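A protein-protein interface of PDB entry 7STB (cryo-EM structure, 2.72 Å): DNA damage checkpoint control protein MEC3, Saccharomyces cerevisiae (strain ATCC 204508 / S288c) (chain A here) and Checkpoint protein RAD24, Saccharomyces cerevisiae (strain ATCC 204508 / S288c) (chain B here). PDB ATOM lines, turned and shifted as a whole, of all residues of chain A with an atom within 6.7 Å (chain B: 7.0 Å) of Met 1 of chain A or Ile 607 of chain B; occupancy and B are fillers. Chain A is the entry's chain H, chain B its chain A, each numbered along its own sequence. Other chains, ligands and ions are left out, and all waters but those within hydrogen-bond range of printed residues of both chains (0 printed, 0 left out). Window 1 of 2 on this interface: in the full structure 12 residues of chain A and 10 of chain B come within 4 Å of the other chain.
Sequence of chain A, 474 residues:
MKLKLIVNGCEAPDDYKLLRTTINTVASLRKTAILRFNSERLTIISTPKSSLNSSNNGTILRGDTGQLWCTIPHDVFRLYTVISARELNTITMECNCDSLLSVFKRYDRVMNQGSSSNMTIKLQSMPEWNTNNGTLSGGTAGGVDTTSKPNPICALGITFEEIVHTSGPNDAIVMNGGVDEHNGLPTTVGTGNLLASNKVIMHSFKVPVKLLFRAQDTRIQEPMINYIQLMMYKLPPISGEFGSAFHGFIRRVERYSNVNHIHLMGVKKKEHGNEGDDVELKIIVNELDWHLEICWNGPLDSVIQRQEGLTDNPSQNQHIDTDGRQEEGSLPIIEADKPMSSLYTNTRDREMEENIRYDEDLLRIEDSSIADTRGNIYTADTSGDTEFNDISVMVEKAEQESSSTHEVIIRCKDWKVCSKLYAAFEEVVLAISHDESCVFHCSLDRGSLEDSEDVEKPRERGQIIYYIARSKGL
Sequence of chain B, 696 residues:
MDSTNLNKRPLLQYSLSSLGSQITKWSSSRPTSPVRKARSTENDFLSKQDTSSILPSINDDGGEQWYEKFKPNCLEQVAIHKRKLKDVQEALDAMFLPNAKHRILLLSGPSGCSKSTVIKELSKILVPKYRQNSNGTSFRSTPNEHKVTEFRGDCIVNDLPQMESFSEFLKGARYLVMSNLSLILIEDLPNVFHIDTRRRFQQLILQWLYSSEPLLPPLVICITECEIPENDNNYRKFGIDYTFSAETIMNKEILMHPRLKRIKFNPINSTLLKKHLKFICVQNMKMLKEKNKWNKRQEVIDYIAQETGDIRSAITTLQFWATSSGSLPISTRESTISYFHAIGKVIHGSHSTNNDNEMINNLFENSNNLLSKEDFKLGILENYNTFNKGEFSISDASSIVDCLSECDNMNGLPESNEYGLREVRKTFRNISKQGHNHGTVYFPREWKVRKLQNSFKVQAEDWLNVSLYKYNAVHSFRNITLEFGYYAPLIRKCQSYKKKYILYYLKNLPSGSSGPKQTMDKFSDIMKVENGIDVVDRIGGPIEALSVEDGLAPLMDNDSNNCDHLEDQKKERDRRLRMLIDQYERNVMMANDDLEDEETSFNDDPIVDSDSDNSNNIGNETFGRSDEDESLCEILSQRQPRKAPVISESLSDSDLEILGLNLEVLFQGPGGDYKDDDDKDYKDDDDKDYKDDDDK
Among the printed residues, pairs that only touch across the chains: Met 1 of chain A with Phe 602 of chain B (3.9 Å), Met 1 of chain A with Ile 607 of chain B (3.2 Å), Lys 2 of chain A with Val 608 of chain B (3.6 Å), Lys 2 of chain A with Ser 610 of chain B (3.8 Å), Ala 85 of chain A with Asp 605 of chain B (3.3 Å), Leu 123 of chain A with Ile 607 of chain B (3.7 Å), Gln 124 of chain A with Ile 607 of chain B (3.5 Å), Gln 124 of chain A with Asp 609 of chain B (3.99 Å), Ser 125 of chain A with Ile 607 of chain B (3.0 Å) and Leu 211 of chain A with Phe 602 of chain B (3.3 Å).
Of the 16 printed residues of chain A, 7 touch a printed residue of chain B.
Hydrophobic or aromatic side chains of chain A that line the printed part of chain B: Met 1, Ala 85 and Leu 211.
Along chain A the printed residues that touch a printed residue of chain B span positions 1 to 211.
Met 1 of chain A touches three residues of chain B.
Of the printed residues of chain B, Gln 124 of chain A touches Ile 607 (3.5 Å) and Asp 609 (3.99 Å).
Of the printed residues of chain B, Leu 211 of chain A touches Phe 602 (3.3 Å).
Of the printed residues of chain A, Asp 605 of chain B touches Ala 85.
Ile 607 of chain B touches just these residues of chain A: Met 1, Leu 123, Gln 124 and Ser 125.
Of the printed residues of chain A, Ser 610 of chain B touches Lys 2.
N of Val 608 of chain B is in hydrogen-bond range of O of Met 1 of chain A (3.0 Å).
The backbone carbonyl oxygen (O) of Ser 601 of chain B sits close to the side-chain carboxylate (OD1) of Asp 605 of chain B, 2.6 Å away.
The side-chain carboxylate (OD1) of Asp 605 of chain B lies close to the backbone carbonyl oxygen (O) of Phe 602 of chain B.
N of Lys 2 of chain A lies within hydrogen-bond range of O of Ile 83 of chain A, at 2.9 Å.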
ATOM      1  N   MET A   1     -12.399 -20.034  18.535  1.00  0.00           N
ATOM      2  CA  MET A   1     -12.247 -18.748  17.796  1.00  0.00           C
ATOM      3  C   MET A   1     -13.145 -18.714  16.563  1.00  0.00           C
ATOM      4  O   MET A   1     -12.933 -19.461  15.609  1.00  0.00           O
ATOM      5  CB  MET A   1     -10.790 -18.537  17.387  1.00  0.00           C
ATOM      6  CG  MET A   1      -9.841 -18.323  18.552  1.00  0.00           C
ATOM      7  SD  MET A   1      -8.126 -18.162  18.021  1.00  0.00           S
ATOM      8  CE  MET A   1      -8.168 -16.560  17.222  1.00  0.00           C
ATOM      9  N   LYS A   2     -14.150 -17.842  16.591  1.00  0.00           N
ATOM     10  CA  LYS A   2     -15.076 -17.669  15.479  1.00  0.00           C
ATOM     11  C   LYS A   2     -15.160 -16.192  15.130  1.00  0.00           C
ATOM     12  O   LYS A   2     -15.377 -15.353  16.010  1.00  0.00           O
ATOM     13  CB  LYS A   2     -16.466 -18.213  15.825  1.00  0.00           C
ATOM     14  CG  LYS A   2     -17.434 -18.227  14.652  1.00  0.00           C
ATOM     15  CD  LYS A   2     -18.863 -18.449  15.115  1.00  0.00           C
ATOM     16  CE  LYS A   2     -19.848 -18.295  13.969  1.00  0.00           C
ATOM     17  NZ  LYS A   2     -21.261 -18.419  14.425  1.00  0.00           N
ATOM     18  N   LEU A   3     -14.990 -15.879  13.847  1.00  0.00           N
ATOM     19  CA  LEU A   3     -15.069 -14.510  13.350  1.00  0.00           C
ATOM     20  C   LEU A   3     -16.025 -14.479  12.167  1.00  0.00           C
ATOM     21  O   LEU A   3     -15.843 -15.226  11.201  1.00  0.00           O
ATOM     22  CB  LEU A   3     -13.687 -13.994  12.939  1.00  0.00           C
ATOM     23  CG  LEU A   3     -13.617 -12.515  12.556  1.00  0.00           C
ATOM     24  CD1 LEU A   3     -13.939 -11.641  13.756  1.00  0.00           C
ATOM     25  CD2 LEU A   3     -12.249 -12.169  11.991  1.00  0.00           C
ATOM     26  N   ILE A  83     -15.975 -14.498  18.721  1.00  0.00           N
ATOM     27  CA  ILE A  83     -15.867 -15.420  19.843  1.00  0.00           C
ATOM     28  C   ILE A  83     -14.414 -15.856  19.953  1.00  0.00           C
ATOM     29  O   ILE A  83     -13.785 -16.191  18.944  1.00  0.00           O
ATOM     30  CB  ILE A  83     -16.792 -16.639  19.667  1.00  0.00           C
ATOM     31  CG1 ILE A  83     -18.259 -16.202  19.696  1.00  0.00           C
ATOM     32  CG2 ILE A  83     -16.529 -17.670  20.752  1.00  0.00           C
ATOM     33  CD1 ILE A  83     -19.185 -17.127  18.939  1.00  0.00           C
ATOM     34  N   SER A  84     -13.882 -15.832  21.171  1.00  0.00           N
ATOM     35  CA  SER A  84     -12.502 -16.235  21.409  1.00  0.00           C
ATOM     36  C   SER A  84     -12.362 -16.644  22.868  1.00  0.00           C
ATOM     37  O   SER A  84     -13.214 -16.338  23.706  1.00  0.00           O
ATOM     38  CB  SER A  84     -11.524 -15.111  21.056  1.00  0.00           C
ATOM     39  OG  SER A  84     -10.186 -15.498  21.320  1.00  0.00           O
ATOM     40  N   ALA A  85     -11.268 -17.342  23.160  1.00  0.00           N
ATOM     41  CA  ALA A  85     -10.974 -17.800  24.510  1.00  0.00           C
ATOM     42  C   ALA A  85     -10.269 -16.748  25.354  1.00  0.00           C
ATOM     43  O   ALA A  85     -10.070 -16.968  26.553  1.00  0.00           O
ATOM     44  CB  ALA A  85     -10.118 -19.070  24.459  1.00  0.00           C
ATOM     45  N   THR A  90     -11.232 -10.965  22.490  1.00  0.00           N
ATOM     46  CA  THR A  90     -10.372 -10.179  21.616  1.00  0.00           C
ATOM     47  C   THR A  90      -9.583 -11.096  20.689  1.00  0.00           C
ATOM     48  O   THR A  90      -8.979 -12.076  21.137  1.00  0.00           O
ATOM     49  CB  THR A  90      -9.415  -9.316  22.437  1.00  0.00           C
ATOM     50  OG1 THR A  90      -8.573 -10.156  23.237  1.00  0.00           O
ATOM     51  CG2 THR A  90     -10.188  -8.359  23.336  1.00  0.00           C
ATOM     52  N   ILE A  91      -9.591 -10.775  19.397  1.00  0.00           N
ATOM     53  CA  ILE A  91      -8.824 -11.503  18.391  1.00  0.00           C
ATOM     54  C   ILE A  91      -7.912 -10.503  17.696  1.00  0.00           C
ATOM     55  O   ILE A  91      -8.391  -9.531  17.101  1.00  0.00           O
ATOM     56  CB  ILE A  91      -9.738 -12.210  17.376  1.00  0.00           C
ATOM     57  CG1 ILE A  91     -10.594 -13.266  18.079  1.00  0.00           C
ATOM     58  CG2 ILE A  91      -8.908 -12.855  16.270  1.00  0.00           C
ATOM     59  CD1 ILE A  91     -11.704 -13.832  17.216  1.00  0.00           C
ATOM     60  N   THR A  92      -6.606 -10.741  17.761  1.00  0.00           N
ATOM     61  CA  THR A  92      -5.615  -9.844  17.183  1.00  0.00           C
ATOM     62  C   THR A  92      -4.999 -10.490  15.951  1.00  0.00           C
ATOM     63  O   THR A  92      -4.606 -11.662  15.988  1.00  0.00           O
ATOM     64  CB  THR A  92      -4.523  -9.500  18.198  1.00  0.00           C
ATOM     65  OG1 THR A  92      -5.124  -9.181  19.459  1.00  0.00           O
ATOM     66  CG2 THR A  92      -3.705  -8.315  17.711  1.00  0.00           C
ATOM     67  N   MET A  93      -4.915  -9.725  14.865  1.00  0.00           N
ATOM     68  CA  MET A  93      -4.426 -10.227  13.591  1.00  0.00           C
ATOM     69  C   MET A  93      -3.487  -9.206  12.967  1.00  0.00           C
ATOM     70  O   MET A  93      -3.597  -8.004  13.216  1.00  0.00           O
ATOM     71  CB  MET A  93      -5.587 -10.519  12.631  1.00  0.00           C
ATOM     72  CG  MET A  93      -6.609 -11.510  13.166  1.00  0.00           C
ATOM     73  SD  MET A  93      -8.218 -11.356  12.370  1.00  0.00           S
ATOM     74  CE  MET A  93      -7.850 -11.967  10.729  1.00  0.00           C
ATOM     75  N   LEU A 123     -12.756 -15.817   9.387  1.00  0.00           N
ATOM     76  CA  LEU A 123     -11.397 -16.271   9.651  1.00  0.00           C
ATOM     77  C   LEU A 123     -11.344 -17.786   9.504  1.00  0.00           C
ATOM     78  O   LEU A 123     -12.116 -18.504  10.148  1.00  0.00           O
ATOM     79  CB  LEU A 123     -10.944 -15.853  11.049  1.00  0.00           C
ATOM     80  CG  LEU A 123      -9.556 -16.329  11.485  1.00  0.00           C
ATOM     81  CD1 LEU A 123      -8.502 -15.926  10.468  1.00  0.00           C
ATOM     82  CD2 LEU A 123      -9.212 -15.777  12.858  1.00  0.00           C
ATOM     83  N   GLN A 124     -10.434 -18.268   8.658  1.00  0.00           N
ATOM     84  CA  GLN A 124     -10.323 -19.685   8.350  1.00  0.00           C
ATOM     85  C   GLN A 124      -8.879 -20.139   8.511  1.00  0.00           C
ATOM     86  O   GLN A 124      -7.941 -19.355   8.351  1.00  0.00           O
ATOM     87  CB  GLN A 124     -10.802 -19.986   6.924  1.00  0.00           C
ATOM     88  CG  GLN A 124     -12.273 -19.679   6.688  1.00  0.00           C
ATOM     89  CD  GLN A 124     -12.582 -19.343   5.242  1.00  0.00           C
ATOM     90  OE1 GLN A 124     -11.681 -19.150   4.427  1.00  0.00           O
ATOM     91  NE2 GLN A 124     -13.868 -19.272   4.916  1.00  0.00           N
ATOM     92  N   SER A 125      -8.713 -21.417   8.832  1.00  0.00           N
ATOM     93  CA  SER A 125      -7.395 -22.020   8.944  1.00  0.00           C
ATOM     94  C   SER A 125      -6.991 -22.599   7.596  1.00  0.00           C
ATOM     95  O   SER A 125      -7.818 -23.142   6.858  1.00  0.00           O
ATOM     96  CB  SER A 125      -7.380 -23.110  10.016  1.00  0.00           C
ATOM     97  OG  SER A 125      -8.225 -24.190   9.660  1.00  0.00           O
ATOM     98  N   MET A 126      -5.703 -22.471   7.276  1.00  0.00           N
ATOM     99  CA  MET A 126      -5.168 -22.854   5.971  1.00  0.00           C
ATOM    100  C   MET A 126      -4.130 -23.952   6.157  1.00  0.00           C
ATOM    101  O   MET A 126      -2.945 -23.666   6.394  1.00  0.00           O
ATOM    102  CB  MET A 126      -4.569 -21.643   5.260  1.00  0.00           C
ATOM    103  CG  MET A 126      -5.595 -20.581   4.891  1.00  0.00           C
ATOM    104  SD  MET A 126      -6.864 -21.192   3.765  1.00  0.00           S
ATOM    105  CE  MET A 126      -5.918 -21.425   2.264  1.00  0.00           C
ATOM    106  N   CYS A 154      -3.316 -17.793   9.162  1.00  0.00           N
ATOM    107  CA  CYS A 154      -4.679 -18.091   8.742  1.00  0.00           C
ATOM    108  C   CYS A 154      -5.062 -17.224   7.550  1.00  0.00           C
ATOM    109  O   CYS A 154      -4.219 -16.506   7.002  1.00  0.00           O
ATOM    110  CB  CYS A 154      -5.647 -17.873   9.906  1.00  0.00           C
ATOM    111  SG  CYS A 154      -5.406 -19.011  11.288  1.00  0.00           S
ATOM    112  N   LEU A 211      -2.070 -14.679  13.041  1.00  0.00           N
ATOM    113  CA  LEU A 211      -2.647 -14.539  14.370  1.00  0.00           C
ATOM    114  C   LEU A 211      -1.569 -14.105  15.354  1.00  0.00           C
ATOM    115  O   LEU A 211      -0.484 -14.692  15.400  1.00  0.00           O
ATOM    116  CB  LEU A 211      -3.282 -15.853  14.818  1.00  0.00           C
ATOM    117  CG  LEU A 211      -4.763 -16.014  14.469  1.00  0.00           C
ATOM    118  CD1 LEU A 211      -4.958 -16.018  12.961  1.00  0.00           C
ATOM    119  CD2 LEU A 211      -5.325 -17.284  15.087  1.00  0.00           C
ATOM    120  N   SER B 601      -2.138 -23.006  23.473  1.00  0.00           N
ATOM    121  CA  SER B 601      -3.431 -22.370  23.703  1.00  0.00           C
ATOM    122  C   SER B 601      -4.251 -22.317  22.421  1.00  0.00           C
ATOM    123  O   SER B 601      -5.451 -22.614  22.431  1.00  0.00           O
ATOM    124  CB  SER B 601      -3.229 -20.964  24.269  1.00  0.00           C
ATOM    125  OG  SER B 601      -4.469 -20.369  24.607  1.00  0.00           O
ATOM    126  N   PHE B 602      -3.621 -21.942  21.306  1.00  0.00           N
ATOM    127  CA  PHE B 602      -4.331 -21.917  20.031  1.00  0.00           C
ATOM    128  C   PHE B 602      -4.793 -23.312  19.634  1.00  0.00           C
ATOM    129  O   PHE B 602      -5.922 -23.490  19.161  1.00  0.00           O
ATOM    130  CB  PHE B 602      -3.436 -21.322  18.944  1.00  0.00           C
ATOM    131  CG  PHE B 602      -4.062 -21.322  17.578  1.00  0.00           C
ATOM    132  CD1 PHE B 602      -5.113 -20.470  17.282  1.00  0.00           C
ATOM    133  CD2 PHE B 602      -3.603 -22.177  16.591  1.00  0.00           C
ATOM    134  CE1 PHE B 602      -5.691 -20.469  16.027  1.00  0.00           C
ATOM    135  CE2 PHE B 602      -4.177 -22.181  15.334  1.00  0.00           C
ATOM    136  CZ  PHE B 602      -5.222 -21.326  15.053  1.00  0.00           C
ATOM    137  N   ASP B 605      -8.024 -24.564  21.248  1.00  0.00           N
ATOM    138  CA  ASP B 605      -9.275 -23.977  20.768  1.00  0.00           C
ATOM    139  C   ASP B 605      -9.183 -23.762  19.263  1.00  0.00           C
ATOM    140  O   ASP B 605      -9.018 -22.631  18.790  1.00  0.00           O
ATOM    141  CB  ASP B 605      -9.578 -22.664  21.494  1.00  0.00           C
ATOM    142  CG  ASP B 605      -8.440 -21.668  21.398  1.00  0.00           C
ATOM    143  OD1 ASP B 605      -7.394 -22.012  20.809  1.00  0.00           O
ATOM    144  OD2 ASP B 605      -8.592 -20.539  21.909  1.00  0.00           O
ATOM    145  N   PRO B 606      -9.283 -24.833  18.477  1.00  0.00           N
ATOM    146  CA  PRO B 606      -9.307 -24.669  17.021  1.00  0.00           C
ATOM    147  C   PRO B 606     -10.479 -23.802  16.589  1.00  0.00           C
ATOM    148  O   PRO B 606     -11.551 -23.819  17.199  1.00  0.00           O
ATOM    149  CB  PRO B 606      -9.444 -26.104  16.500  1.00  0.00           C
ATOM    150  CG  PRO B 606      -8.950 -26.965  17.613  1.00  0.00           C
ATOM    151  CD  PRO B 606      -9.337 -26.252  18.871  1.00  0.00           C
ATOM    152  N   ILE B 607     -10.262 -23.031  15.522  1.00  0.00           N
ATOM    153  CA  ILE B 607     -11.301 -22.128  15.052  1.00  0.00           C
ATOM    154  C   ILE B 607     -12.552 -22.925  14.688  1.00  0.00           C
ATOM    155  O   ILE B 607     -12.514 -24.143  14.474  1.00  0.00           O
ATOM    156  CB  ILE B 607     -10.816 -21.301  13.851  1.00  0.00           C
ATOM    157  CG1 ILE B 607     -10.479 -22.220  12.677  1.00  0.00           C
ATOM    158  CG2 ILE B 607      -9.589 -20.480  14.225  1.00  0.00           C
ATOM    159  CD1 ILE B 607     -10.226 -21.484  11.404  1.00  0.00           C
ATOM    160  N   VAL B 608     -13.677 -22.220  14.617  1.00  0.00           N
ATOM    161  CA  VAL B 608     -14.960 -22.803  14.239  1.00  0.00           C
ATOM    162  C   VAL B 608     -15.431 -22.110  12.969  1.00  0.00           C
ATOM    163  O   VAL B 608     -15.714 -20.906  12.980  1.00  0.00           O
ATOM    164  CB  VAL B 608     -16.003 -22.665  15.358  1.00  0.00           C
ATOM    165  CG1 VAL B 608     -17.306 -23.337  14.952  1.00  0.00           C
ATOM    166  CG2 VAL B 608     -15.474 -23.257  16.654  1.00  0.00           C
ATOM    167  N   ASP B 609     -15.520 -22.870  11.879  1.00  0.00           N
ATOM    168  CA  ASP B 609     -16.001 -22.345  10.603  1.00  0.00           C
ATOM    169  C   ASP B 609     -17.484 -22.681  10.444  1.00  0.00           C
ATOM    170  O   ASP B 609     -17.884 -23.566   9.686  1.00  0.00           O
ATOM    171  CB  ASP B 609     -15.168 -22.906   9.453  1.00  0.00           C
ATOM    172  CG  ASP B 609     -15.472 -22.230   8.129  1.00  0.00           C
ATOM    173  OD1 ASP B 609     -16.281 -21.278   8.118  1.00  0.00           O
ATOM    174  OD2 ASP B 609     -14.902 -22.651   7.101  1.00  0.00           O
ATOM    175  N   SER B 610     -18.302 -21.943  11.188  1.00  0.00           N
ATOM    176  CA  SER B 610     -19.746 -22.130  11.194  1.00  0.00           C
ATOM    177  C   SER B 610     -20.405 -21.053  10.344  1.00  0.00           C
ATOM    178  O   SER B 610     -20.171 -19.859  10.553  1.00  0.00           O
ATOM    179  CB  SER B 610     -20.294 -22.084  12.622  1.00  0.00           C
ATOM    180  OG  SER B 610     -21.709 -22.175  12.627  1.00  0.00           O
